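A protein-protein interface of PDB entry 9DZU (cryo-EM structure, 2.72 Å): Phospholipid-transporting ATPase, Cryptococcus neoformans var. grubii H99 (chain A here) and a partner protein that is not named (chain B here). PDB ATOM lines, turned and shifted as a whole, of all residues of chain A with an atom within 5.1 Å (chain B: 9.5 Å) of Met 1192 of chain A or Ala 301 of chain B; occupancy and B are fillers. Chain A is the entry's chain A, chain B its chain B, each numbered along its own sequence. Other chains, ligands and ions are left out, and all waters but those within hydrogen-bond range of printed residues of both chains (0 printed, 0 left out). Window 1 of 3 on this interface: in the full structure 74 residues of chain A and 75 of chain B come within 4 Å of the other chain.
Among the printed residues, pairs that only touch across the chains: Asn 1172 of chain A with Leu 302 of chain B (3.2 Å), Tyr 1188 of chain A with Arg 298 of chain B (3.2 Å), Phe 1088 of chain A with Ala 301 of chain B (3.4 Å), Tyr 1188 of chain A with Val 299 of chain B (3.4 Å), Met 1192 of chain A with Ala 301 of chain B (3.7 Å), Met 1189 of chain A with Ala 301 of chain B (3.7 Å) and Phe 1088 of chain A with Asn 167 of chain B (3.8 Å).
Of chain B, only Ala 301 comes within 4 Å of Met 1192 of chain A. Of the printed residues of chain B, Tyr 1188 of chain A touches Arg 298 (3.2 Å) and Val 299 (3.4 Å). Printed residues of chain B within 4 Å of Asn 1172 of chain A: Leu 302. Phe 305 of chain B touches none of the printed residues of chain A. The nearest printed residue of chain A that does not touch Leu 302 of chain B is Met 1192 of chain A (4.5 Å).
N of Met 1189 of chain A lies within hydrogen-bond range of O of Val 299 of chain B (2.9 Å).
The side-chain amide nitrogen of Asn 167 of chain B sits at hydrogen-bond distance from the backbone carbonyl oxygen of Ala 301 of chain B (3.0 Å). The backbone carbonyl oxygen (O) of Arg 298 of chain B sits at hydrogen-bond distance from the side-chain amino group (NZ) of Lys 307 of chain B, at 2.7 Å. The backbone carbonyl oxygen (O) of Met 1189 of chain A is in hydrogen-bond range of the side-chain hydroxyl (OG) of Ser 1193 of chain A. SD of Met 1192 of chain A sits close to NE2 of Gln 1196 of chain A, at 3.5 Å.
Hydrophobic or aromatic side chains of chain A that line the printed part of chain B: Phe 1088, Tyr 1188, Met 1189 and Met 1192. Printed residues of chain B that touch a printed residue of chain A: Asn 167, Arg 298, Val 299, Ala 301 and Leu 302. Hydrophobic or aromatic side chains of chain B within 4 Å of the printed part of chain A: Ala 301 and Leu 302. Among the printed residues, no Asp or Glu carboxylate lies within 4 Å of a Lys or Arg side-chain nitrogen of the other chain.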
ATOM      1  N   PHE A1088     -18.132 -17.297  23.674  1.00  0.00           N
ATOM      2  CA  PHE A1088     -19.123 -18.037  22.898  1.00  0.00           C
ATOM      3  C   PHE A1088     -20.138 -17.096  22.268  1.00  0.00           C
ATOM      4  O   PHE A1088     -20.576 -17.318  21.133  1.00  0.00           O
ATOM      5  CB  PHE A1088     -19.844 -19.073  23.745  1.00  0.00           C
ATOM      6  CG  PHE A1088     -20.919 -19.795  22.989  1.00  0.00           C
ATOM      7  CD1 PHE A1088     -20.589 -20.695  21.994  1.00  0.00           C
ATOM      8  CD2 PHE A1088     -22.253 -19.557  23.251  1.00  0.00           C
ATOM      9  CE1 PHE A1088     -21.569 -21.354  21.287  1.00  0.00           C
ATOM     10  CE2 PHE A1088     -23.235 -20.218  22.548  1.00  0.00           C
ATOM     11  CZ  PHE A1088     -22.892 -21.115  21.565  1.00  0.00           C
ATOM     12  N   VAL A1099     -23.555 -21.180  26.676  1.00  0.00           N
ATOM     13  CA  VAL A1099     -22.799 -22.280  26.084  1.00  0.00           C
ATOM     14  C   VAL A1099     -22.811 -23.482  27.019  1.00  0.00           C
ATOM     15  O   VAL A1099     -23.114 -24.607  26.610  1.00  0.00           O
ATOM     16  CB  VAL A1099     -21.365 -21.833  25.741  1.00  0.00           C
ATOM     17  CG1 VAL A1099     -20.759 -21.023  26.874  1.00  0.00           C
ATOM     18  CG2 VAL A1099     -20.494 -23.032  25.413  1.00  0.00           C
ATOM     19  N   TYR A1168     -11.756 -20.969  25.623  1.00  0.00           N
ATOM     20  CA  TYR A1168     -12.839 -21.088  24.657  1.00  0.00           C
ATOM     21  C   TYR A1168     -12.306 -21.275  23.248  1.00  0.00           C
ATOM     22  O   TYR A1168     -12.748 -22.176  22.531  1.00  0.00           O
ATOM     23  CB  TYR A1168     -13.759 -19.869  24.703  1.00  0.00           C
ATOM     24  CG  TYR A1168     -14.811 -19.941  23.622  1.00  0.00           C
ATOM     25  CD1 TYR A1168     -15.945 -20.719  23.787  1.00  0.00           C
ATOM     26  CD2 TYR A1168     -14.647 -19.271  22.419  1.00  0.00           C
ATOM     27  CE1 TYR A1168     -16.893 -20.812  22.798  1.00  0.00           C
ATOM     28  CE2 TYR A1168     -15.592 -19.359  21.425  1.00  0.00           C
ATOM     29  CZ  TYR A1168     -16.713 -20.128  21.619  1.00  0.00           C
ATOM     30  OH  TYR A1168     -17.661 -20.212  20.626  1.00  0.00           O
ATOM     31  N   LEU A1171     -10.411 -24.722  22.601  1.00  0.00           N
ATOM     32  CA  LEU A1171     -11.305 -25.876  22.601  1.00  0.00           C
ATOM     33  C   LEU A1171     -12.324 -25.808  21.467  1.00  0.00           C
ATOM     34  O   LEU A1171     -12.713 -26.848  20.922  1.00  0.00           O
ATOM     35  CB  LEU A1171     -11.990 -26.003  23.957  1.00  0.00           C
ATOM     36  CG  LEU A1171     -11.009 -26.475  25.028  1.00  0.00           C
ATOM     37  CD1 LEU A1171     -11.642 -26.496  26.398  1.00  0.00           C
ATOM     38  CD2 LEU A1171     -10.472 -27.847  24.670  1.00  0.00           C
ATOM     39  N   ASN A1172     -12.742 -24.603  21.076  1.00  0.00           N
ATOM     40  CA  ASN A1172     -13.662 -24.453  19.956  1.00  0.00           C
ATOM     41  C   ASN A1172     -13.027 -24.928  18.658  1.00  0.00           C
ATOM     42  O   ASN A1172     -13.598 -25.759  17.941  1.00  0.00           O
ATOM     43  CB  ASN A1172     -14.092 -22.990  19.843  1.00  0.00           C
ATOM     44  CG  ASN A1172     -14.871 -22.703  18.579  1.00  0.00           C
ATOM     45  OD1 ASN A1172     -15.579 -23.564  18.062  1.00  0.00           O
ATOM     46  ND2 ASN A1172     -14.741 -21.485  18.073  1.00  0.00           N
ATOM     47  N   TYR A1175     -12.841 -28.617  18.594  1.00  0.00           N
ATOM     48  CA  TYR A1175     -14.097 -29.307  18.335  1.00  0.00           C
ATOM     49  C   TYR A1175     -14.727 -28.937  17.001  1.00  0.00           C
ATOM     50  O   TYR A1175     -15.812 -29.438  16.690  1.00  0.00           O
ATOM     51  CB  TYR A1175     -15.094 -29.038  19.465  1.00  0.00           C
ATOM     52  CG  TYR A1175     -14.915 -29.944  20.658  1.00  0.00           C
ATOM     53  CD1 TYR A1175     -15.449 -31.221  20.666  1.00  0.00           C
ATOM     54  CD2 TYR A1175     -14.217 -29.520  21.778  1.00  0.00           C
ATOM     55  CE1 TYR A1175     -15.292 -32.050  21.749  1.00  0.00           C
ATOM     56  CE2 TYR A1175     -14.055 -30.343  22.866  1.00  0.00           C
ATOM     57  CZ  TYR A1175     -14.595 -31.605  22.847  1.00  0.00           C
ATOM     58  OH  TYR A1175     -14.435 -32.431  23.934  1.00  0.00           O
ATOM     59  N   VAL A1187     -20.598 -33.680  17.071  1.00  0.00           N
ATOM     60  CA  VAL A1187     -20.191 -32.800  18.157  1.00  0.00           C
ATOM     61  C   VAL A1187     -21.302 -31.788  18.384  1.00  0.00           C
ATOM     62  O   VAL A1187     -21.482 -30.862  17.584  1.00  0.00           O
ATOM     63  CB  VAL A1187     -18.864 -32.095  17.842  1.00  0.00           C
ATOM     64  CG1 VAL A1187     -18.514 -31.116  18.945  1.00  0.00           C
ATOM     65  CG2 VAL A1187     -17.755 -33.113  17.656  1.00  0.00           C
ATOM     66  N   TYR A1188     -22.051 -31.959  19.465  1.00  0.00           N
ATOM     67  CA  TYR A1188     -23.076 -31.002  19.846  1.00  0.00           C
ATOM     68  C   TYR A1188     -22.505 -30.037  20.881  1.00  0.00           C
ATOM     69  O   TYR A1188     -21.373 -30.184  21.345  1.00  0.00           O
ATOM     70  CB  TYR A1188     -24.336 -31.717  20.342  1.00  0.00           C
ATOM     71  CG  TYR A1188     -24.233 -32.408  21.679  1.00  0.00           C
ATOM     72  CD1 TYR A1188     -23.460 -33.546  21.841  1.00  0.00           C
ATOM     73  CD2 TYR A1188     -24.950 -31.946  22.771  1.00  0.00           C
ATOM     74  CE1 TYR A1188     -23.386 -34.186  23.058  1.00  0.00           C
ATOM     75  CE2 TYR A1188     -24.881 -32.580  23.988  1.00  0.00           C
ATOM     76  CZ  TYR A1188     -24.095 -33.697  24.129  1.00  0.00           C
ATOM     77  OH  TYR A1188     -24.024 -34.330  25.347  1.00  0.00           O
ATOM     78  N   MET A1189     -23.311 -29.036  21.235  1.00  0.00           N
ATOM     79  CA  MET A1189     -22.792 -27.889  21.975  1.00  0.00           C
ATOM     80  C   MET A1189     -22.256 -28.292  23.342  1.00  0.00           C
ATOM     81  O   MET A1189     -21.226 -27.772  23.789  1.00  0.00           O
ATOM     82  CB  MET A1189     -23.881 -26.825  22.117  1.00  0.00           C
ATOM     83  CG  MET A1189     -23.412 -25.533  22.762  1.00  0.00           C
ATOM     84  SD  MET A1189     -24.659 -24.234  22.706  1.00  0.00           S
ATOM     85  CE  MET A1189     -25.998 -25.014  23.603  1.00  0.00           C
ATOM     86  N   TYR A1190     -22.932 -29.217  24.021  1.00  0.00           N
ATOM     87  CA  TYR A1190     -22.605 -29.482  25.415  1.00  0.00           C
ATOM     88  C   TYR A1190     -21.327 -30.292  25.601  1.00  0.00           C
ATOM     89  O   TYR A1190     -20.730 -30.210  26.673  1.00  0.00           O
ATOM     90  CB  TYR A1190     -23.778 -30.174  26.108  1.00  0.00           C
ATOM     91  CG  TYR A1190     -24.937 -29.241  26.377  1.00  0.00           C
ATOM     92  CD1 TYR A1190     -24.753 -27.868  26.398  1.00  0.00           C
ATOM     93  CD2 TYR A1190     -26.212 -29.733  26.609  1.00  0.00           C
ATOM     94  CE1 TYR A1190     -25.802 -27.009  26.643  1.00  0.00           C
ATOM     95  CE2 TYR A1190     -27.269 -28.879  26.856  1.00  0.00           C
ATOM     96  CZ  TYR A1190     -27.056 -27.518  26.871  1.00  0.00           C
ATOM     97  OH  TYR A1190     -28.102 -26.660  27.115  1.00  0.00           O
ATOM     98  N   GLU A1191     -20.868 -31.038  24.593  1.00  0.00           N
ATOM     99  CA  GLU A1191     -19.549 -31.663  24.701  1.00  0.00           C
ATOM    100  C   GLU A1191     -18.460 -30.609  24.852  1.00  0.00           C
ATOM    101  O   GLU A1191     -17.672 -30.630  25.812  1.00  0.00           O
ATOM    102  CB  GLU A1191     -19.267 -32.527  23.475  1.00  0.00           C
ATOM    103  CG  GLU A1191     -20.021 -33.832  23.420  1.00  0.00           C
ATOM    104  CD  GLU A1191     -19.684 -34.630  22.179  1.00  0.00           C
ATOM    105  OE1 GLU A1191     -18.598 -34.406  21.607  1.00  0.00           O
ATOM    106  OE2 GLU A1191     -20.507 -35.477  21.770  1.00  0.00           O
ATOM    107  N   MET A1192     -18.418 -29.664  23.911  1.00  0.00           N
ATOM    108  CA  MET A1192     -17.455 -28.575  23.981  1.00  0.00           C
ATOM    109  C   MET A1192     -17.684 -27.736  25.226  1.00  0.00           C
ATOM    110  O   MET A1192     -16.727 -27.292  25.871  1.00  0.00           O
ATOM    111  CB  MET A1192     -17.563 -27.717  22.723  1.00  0.00           C
ATOM    112  CG  MET A1192     -16.511 -26.639  22.599  1.00  0.00           C
ATOM    113  SD  MET A1192     -16.898 -25.487  21.271  1.00  0.00           S
ATOM    114  CE  MET A1192     -18.370 -24.705  21.920  1.00  0.00           C
ATOM    115  N   SER A1193     -18.949 -27.517  25.584  1.00  0.00           N
ATOM    116  CA  SER A1193     -19.265 -26.723  26.763  1.00  0.00           C
ATOM    117  C   SER A1193     -18.712 -27.360  28.030  1.00  0.00           C
ATOM    118  O   SER A1193     -18.136 -26.672  28.875  1.00  0.00           O
ATOM    119  CB  SER A1193     -20.776 -26.549  26.877  1.00  0.00           C
ATOM    120  OG  SER A1193     -21.334 -26.122  25.648  1.00  0.00           O
ATOM    121  N   THR A1194     -18.879 -28.675  28.183  1.00  0.00           N
ATOM    122  CA  THR A1194     -18.411 -29.342  29.389  1.00  0.00           C
ATOM    123  C   THR A1194     -16.891 -29.414  29.421  1.00  0.00           C
ATOM    124  O   THR A1194     -16.281 -29.261  30.487  1.00  0.00           O
ATOM    125  CB  THR A1194     -19.023 -30.736  29.489  1.00  0.00           C
ATOM    126  OG1 THR A1194     -20.423 -30.663  29.199  1.00  0.00           O
ATOM    127  CG2 THR A1194     -18.840 -31.293  30.889  1.00  0.00           C
ATOM    128  N   THR A1195     -16.258 -29.631  28.264  1.00  0.00           N
ATOM    129  CA  THR A1195     -14.799 -29.587  28.226  1.00  0.00           C
ATOM    130  C   THR A1195     -14.286 -28.213  28.641  1.00  0.00           C
ATOM    131  O   THR A1195     -13.356 -28.103  29.452  1.00  0.00           O
ATOM    132  CB  THR A1195     -14.293 -29.955  26.833  1.00  0.00           C
ATOM    133  OG1 THR A1195     -14.750 -31.268  26.489  1.00  0.00           O
ATOM    134  CG2 THR A1195     -12.781 -29.939  26.798  1.00  0.00           C
ATOM    135  N   GLN A1196     -14.906 -27.150  28.120  1.00  0.00           N
ATOM    136  CA  GLN A1196     -14.503 -25.796  28.481  1.00  0.00           C
ATOM    137  C   GLN A1196     -14.767 -25.507  29.952  1.00  0.00           C
ATOM    138  O   GLN A1196     -13.970 -24.830  30.606  1.00  0.00           O
ATOM    139  CB  GLN A1196     -15.228 -24.785  27.596  1.00  0.00           C
ATOM    140  CG  GLN A1196     -14.798 -24.829  26.145  1.00  0.00           C
ATOM    141  CD  GLN A1196     -15.666 -23.985  25.247  1.00  0.00           C
ATOM    142  OE1 GLN A1196     -16.671 -23.427  25.682  1.00  0.00           O
ATOM    143  NE2 GLN A1196     -15.285 -23.885  23.982  1.00  0.00           N
ATOM    144  N   ALA A1197     -15.884 -26.000  30.489  1.00  0.00           N
ATOM    145  CA  ALA A1197     -16.197 -25.765  31.895  1.00  0.00           C
ATOM    146  C   ALA A1197     -15.193 -26.450  32.808  1.00  0.00           C
ATOM    147  O   ALA A1197     -14.737 -25.861  33.797  1.00  0.00           O
ATOM    148  CB  ALA A1197     -17.615 -26.241  32.202  1.00  0.00           C
ATOM    149  N   LEU B 161     -24.171 -27.931   7.414  1.00  0.00           N
ATOM    150  CA  LEU B 161     -24.993 -26.745   7.222  1.00  0.00           C
ATOM    151  C   LEU B 161     -24.210 -25.520   7.664  1.00  0.00           C
ATOM    152  O   LEU B 161     -23.724 -25.464   8.798  1.00  0.00           O
ATOM    153  CB  LEU B 161     -26.303 -26.847   8.001  1.00  0.00           C
ATOM    154  CG  LEU B 161     -27.292 -27.907   7.519  1.00  0.00           C
ATOM    155  CD1 LEU B 161     -28.526 -27.910   8.384  1.00  0.00           C
ATOM    156  CD2 LEU B 161     -27.662 -27.661   6.077  1.00  0.00           C
ATOM    157  N   TYR B 164     -26.207 -21.641   9.717  1.00  0.00           N
ATOM    158  CA  TYR B 164     -27.398 -22.185  10.362  1.00  0.00           C
ATOM    159  C   TYR B 164     -27.205 -22.057  11.867  1.00  0.00           C
ATOM    160  O   TYR B 164     -26.518 -22.876  12.485  1.00  0.00           O
ATOM    161  CB  TYR B 164     -27.641 -23.632   9.952  1.00  0.00           C
ATOM    162  CG  TYR B 164     -29.069 -24.077  10.143  1.00  0.00           C
ATOM    163  CD1 TYR B 164     -29.576 -24.322  11.410  1.00  0.00           C
ATOM    164  CD2 TYR B 164     -29.908 -24.257   9.057  1.00  0.00           C
ATOM    165  CE1 TYR B 164     -30.877 -24.726  11.587  1.00  0.00           C
ATOM    166  CE2 TYR B 164     -31.209 -24.664   9.227  1.00  0.00           C
ATOM    167  CZ  TYR B 164     -31.689 -24.897  10.494  1.00  0.00           C
ATOM    168  OH  TYR B 164     -32.989 -25.304  10.669  1.00  0.00           O
ATOM    169  N   TYR B 165     -27.819 -21.035  12.457  1.00  0.00           N
ATOM    170  CA  TYR B 165     -27.632 -20.724  13.872  1.00  0.00           C
ATOM    171  C   TYR B 165     -28.601 -21.556  14.704  1.00  0.00           C
ATOM    172  O   TYR B 165     -29.707 -21.134  15.046  1.00  0.00           O
ATOM    173  CB  TYR B 165     -27.810 -19.233  14.116  1.00  0.00           C
ATOM    174  CG  TYR B 165     -26.664 -18.400  13.601  1.00  0.00           C
ATOM    175  CD1 TYR B 165     -26.573 -18.062  12.261  1.00  0.00           C
ATOM    176  CD2 TYR B 165     -25.668 -17.958  14.455  1.00  0.00           C
ATOM    177  CE1 TYR B 165     -25.523 -17.307  11.789  1.00  0.00           C
ATOM    178  CE2 TYR B 165     -24.615 -17.203  13.992  1.00  0.00           C
ATOM    179  CZ  TYR B 165     -24.548 -16.880  12.659  1.00  0.00           C
ATOM    180  OH  TYR B 165     -23.498 -16.125  12.192  1.00  0.00           O
ATOM    181  N   GLN B 166     -28.170 -22.775  15.031  1.00  0.00           N
ATOM    182  CA  GLN B 166     -28.890 -23.573  16.012  1.00  0.00           C
ATOM    183  C   GLN B 166     -28.625 -23.102  17.434  1.00  0.00           C
ATOM    184  O   GLN B 166     -29.390 -23.444  18.340  1.00  0.00           O
ATOM    185  CB  GLN B 166     -28.518 -25.048  15.888  1.00  0.00           C
ATOM    186  CG  GLN B 166     -29.315 -25.811  14.859  1.00  0.00           C
ATOM    187  CD  GLN B 166     -29.352 -27.294  15.150  1.00  0.00           C
ATOM    188  OE1 GLN B 166     -28.401 -27.853  15.692  1.00  0.00           O
ATOM    189  NE2 GLN B 166     -30.455 -27.939  14.802  1.00  0.00           N
ATOM    190  N   ASN B 167     -27.571 -22.322  17.642  1.00  0.00           N
ATOM    191  CA  ASN B 167     -27.185 -21.855  18.963  1.00  0.00           C
ATOM    192  C   ASN B 167     -27.871 -20.557  19.355  1.00  0.00           C
ATOM    193  O   ASN B 167     -27.582 -20.020  20.428  1.00  0.00           O
ATOM    194  CB  ASN B 167     -25.666 -21.688  19.030  1.00  0.00           C
ATOM    195  CG  ASN B 167     -25.098 -21.053  17.781  1.00  0.00           C
ATOM    196  OD1 ASN B 167     -25.757 -20.996  16.746  1.00  0.00           O
ATOM    197  ND2 ASN B 167     -23.863 -20.581  17.867  1.00  0.00           N
ATOM    198  N   HIS B 168     -28.767 -20.042  18.521  1.00  0.00           N
ATOM    199  CA  HIS B 168     -29.525 -18.852  18.876  1.00  0.00           C
ATOM    200  C   HIS B 168     -30.422 -19.142  20.072  1.00  0.00           C
ATOM    201  O   HIS B 168     -30.909 -20.260  20.254  1.00  0.00           O
ATOM    202  CB  HIS B 168     -30.357 -18.379  17.688  1.00  0.00           C
ATOM    203  CG  HIS B 168     -30.759 -16.940  17.763  1.00  0.00           C
ATOM    204  ND1 HIS B 168     -31.958 -16.529  18.301  1.00  0.00           N
ATOM    205  CD2 HIS B 168     -30.125 -15.817  17.356  1.00  0.00           C
ATOM    206  CE1 HIS B 168     -32.043 -15.213  18.229  1.00  0.00           C
ATOM    207  NE2 HIS B 168     -30.942 -14.756  17.661  1.00  0.00           N
ATOM    208  N   SER B 172     -32.288 -22.565  20.567  1.00  0.00           N
ATOM    209  CA  SER B 172     -31.574 -23.555  21.369  1.00  0.00           C
ATOM    210  C   SER B 172     -32.452 -24.157  22.457  1.00  0.00           C
ATOM    211  O   SER B 172     -32.240 -25.308  22.853  1.00  0.00           O
ATOM    212  CB  SER B 172     -30.325 -22.926  21.984  1.00  0.00           C
ATOM    213  OG  SER B 172     -30.660 -21.805  22.782  1.00  0.00           O
ATOM    214  N   ARG B 298     -30.213 -32.482  18.827  1.00  0.00           N
ATOM    215  CA  ARG B 298     -28.998 -32.102  19.539  1.00  0.00           C
ATOM    216  C   ARG B 298     -28.462 -30.799  18.961  1.00  0.00           C
ATOM    217  O   ARG B 298     -27.993 -30.762  17.820  1.00  0.00           O
ATOM    218  CB  ARG B 298     -27.961 -33.216  19.440  1.00  0.00           C
ATOM    219  CG  ARG B 298     -28.216 -34.374  20.382  1.00  0.00           C
ATOM    220  CD  ARG B 298     -27.741 -35.685  19.789  1.00  0.00           C
ATOM    221  NE  ARG B 298     -26.333 -35.649  19.418  1.00  0.00           N
ATOM    222  CZ  ARG B 298     -25.338 -35.981  20.225  1.00  0.00           C
ATOM    223  NH1 ARG B 298     -25.558 -36.364  21.472  1.00  0.00           N
ATOM    224  NH2 ARG B 298     -24.089 -35.928  19.772  1.00  0.00           N
ATOM    225  N   VAL B 299     -28.531 -29.728  19.750  1.00  0.00           N
ATOM    226  CA  VAL B 299     -28.170 -28.403  19.264  1.00  0.00           C
ATOM    227  C   VAL B 299     -26.671 -28.336  19.011  1.00  0.00           C
ATOM    228  O   VAL B 299     -25.861 -28.741  19.855  1.00  0.00           O
ATOM    229  CB  VAL B 299     -28.618 -27.328  20.264  1.00  0.00           C
ATOM    230  CG1 VAL B 299     -28.080 -25.971  19.860  1.00  0.00           C
ATOM    231  CG2 VAL B 299     -30.133 -27.298  20.356  1.00  0.00           C
ATOM    232  N   ALA B 300     -26.298 -27.820  17.844  1.00  0.00           N
ATOM    233  CA  ALA B 300     -24.900 -27.686  17.473  1.00  0.00           C
ATOM    234  C   ALA B 300     -24.288 -26.433  18.084  1.00  0.00           C
ATOM    235  O   ALA B 300     -24.977 -25.449  18.364  1.00  0.00           O
ATOM    236  CB  ALA B 300     -24.757 -27.644  15.956  1.00  0.00           C
ATOM    237  N   ALA B 301     -22.971 -26.481  18.291  1.00  0.00           N
ATOM    238  CA  ALA B 301     -22.274 -25.385  18.952  1.00  0.00           C
ATOM    239  C   ALA B 301     -22.096 -24.180  18.038  1.00  0.00           C
ATOM    240  O   ALA B 301     -22.268 -23.038  18.475  1.00  0.00           O
ATOM    241  CB  ALA B 301     -20.918 -25.865  19.466  1.00  0.00           C
ATOM    242  N   LEU B 302     -21.759 -24.408  16.777  1.00  0.00           N
ATOM    243  CA  LEU B 302     -21.409 -23.352  15.842  1.00  0.00           C
ATOM    244  C   LEU B 302     -22.375 -23.338  14.664  1.00  0.00           C
ATOM    245  O   LEU B 302     -23.016 -24.352  14.364  1.00  0.00           O
ATOM    246  CB  LEU B 302     -19.972 -23.532  15.332  1.00  0.00           C
ATOM    247  CG  LEU B 302     -18.831 -22.980  16.190  1.00  0.00           C
ATOM    248  CD1 LEU B 302     -18.696 -23.738  17.496  1.00  0.00           C
ATOM    249  CD2 LEU B 302     -17.523 -23.010  15.414  1.00  0.00           C
ATOM    250  N   PRO B 303     -22.519 -22.196  13.985  1.00  0.00           N
ATOM    251  CA  PRO B 303     -23.393 -22.158  12.802  1.00  0.00           C
ATOM    252  C   PRO B 303     -22.982 -23.128  11.711  1.00  0.00           C
ATOM    253  O   PRO B 303     -23.853 -23.660  11.012  1.00  0.00           O
ATOM    254  CB  PRO B 303     -23.289 -20.699  12.335  1.00  0.00           C
ATOM    255  CG  PRO B 303     -22.066 -20.161  12.993  1.00  0.00           C
ATOM    256  CD  PRO B 303     -21.973 -20.867  14.300  1.00  0.00           C
ATOM    257  N   THR B 304     -21.687 -23.374  11.537  1.00  0.00           N
ATOM    258  CA  THR B 304     -21.206 -24.382  10.598  1.00  0.00           C
ATOM    259  C   THR B 304     -21.044 -25.691  11.358  1.00  0.00           C
ATOM    260  O   THR B 304     -20.131 -25.832  12.176  1.00  0.00           O
ATOM    261  CB  THR B 304     -19.890 -23.951   9.958  1.00  0.00           C
ATOM    262  OG1 THR B 304     -20.077 -22.713   9.264  1.00  0.00           O
ATOM    263  CG2 THR B 304     -19.412 -25.004   8.978  1.00  0.00           C
ATOM    264  N   PHE B 305     -21.931 -26.646  11.095  1.00  0.00           N
ATOM    265  CA  PHE B 305     -21.939 -27.896  11.837  1.00  0.00           C
ATOM    266  C   PHE B 305     -22.245 -29.057  10.907  1.00  0.00           C
ATOM    267  O   PHE B 305     -22.834 -28.890   9.837  1.00  0.00           O
ATOM    268  CB  PHE B 305     -22.953 -27.866  12.987  1.00  0.00           C
ATOM    269  CG  PHE B 305     -24.371 -27.636  12.549  1.00  0.00           C
ATOM    270  CD1 PHE B 305     -25.199 -28.701  12.242  1.00  0.00           C
ATOM    271  CD2 PHE B 305     -24.883 -26.354  12.463  1.00  0.00           C
ATOM    272  CE1 PHE B 305     -26.499 -28.490  11.845  1.00  0.00           C
ATOM    273  CE2 PHE B 305     -26.184 -26.141  12.069  1.00  0.00           C
ATOM    274  CZ  PHE B 305     -26.991 -27.211  11.760  1.00  0.00           C
ATOM    275  N   ARG B 306     -21.837 -30.245  11.339  1.00  0.00           N
ATOM    276  CA  ARG B 306     -22.038 -31.478  10.594  1.00  0.00           C
ATOM    277  C   ARG B 306     -22.834 -32.441  11.459  1.00  0.00           C
ATOM    278  O   ARG B 306     -22.525 -32.615  12.641  1.00  0.00           O
ATOM    279  CB  ARG B 306     -20.699 -32.101  10.192  1.00  0.00           C
ATOM    280  CG  ARG B 306     -19.758 -31.143   9.494  1.00  0.00           C
ATOM    281  CD  ARG B 306     -18.415 -31.093  10.191  1.00  0.00           C
ATOM    282  NE  ARG B 306     -17.506 -30.141   9.565  1.00  0.00           N
ATOM    283  CZ  ARG B 306     -17.305 -28.904   9.996  1.00  0.00           C
ATOM    284  NH1 ARG B 306     -17.936 -28.431  11.057  1.00  0.00           N
ATOM    285  NH2 ARG B 306     -16.449 -28.123   9.346  1.00  0.00           N
ATOM    286  N   LYS B 307     -23.857 -33.055  10.876  1.00  0.00           N
ATOM    287  CA  LYS B 307     -24.691 -34.023  11.573  1.00  0.00           C
ATOM    288  C   LYS B 307     -24.695 -35.339  10.810  1.00  0.00           C
ATOM    289  O   LYS B 307     -24.792 -35.357   9.579  1.00  0.00           O
ATOM    290  CB  LYS B 307     -26.116 -33.501  11.752  1.00  0.00           C
ATOM    291  CG  LYS B 307     -26.212 -32.347  12.731  1.00  0.00           C
ATOM    292  CD  LYS B 307     -27.649 -31.988  13.039  1.00  0.00           C
ATOM    293  CE  LYS B 307     -27.724 -30.951  14.139  1.00  0.00           C
ATOM    294  NZ  LYS B 307     -27.072 -31.426  15.386  1.00  0.00           N
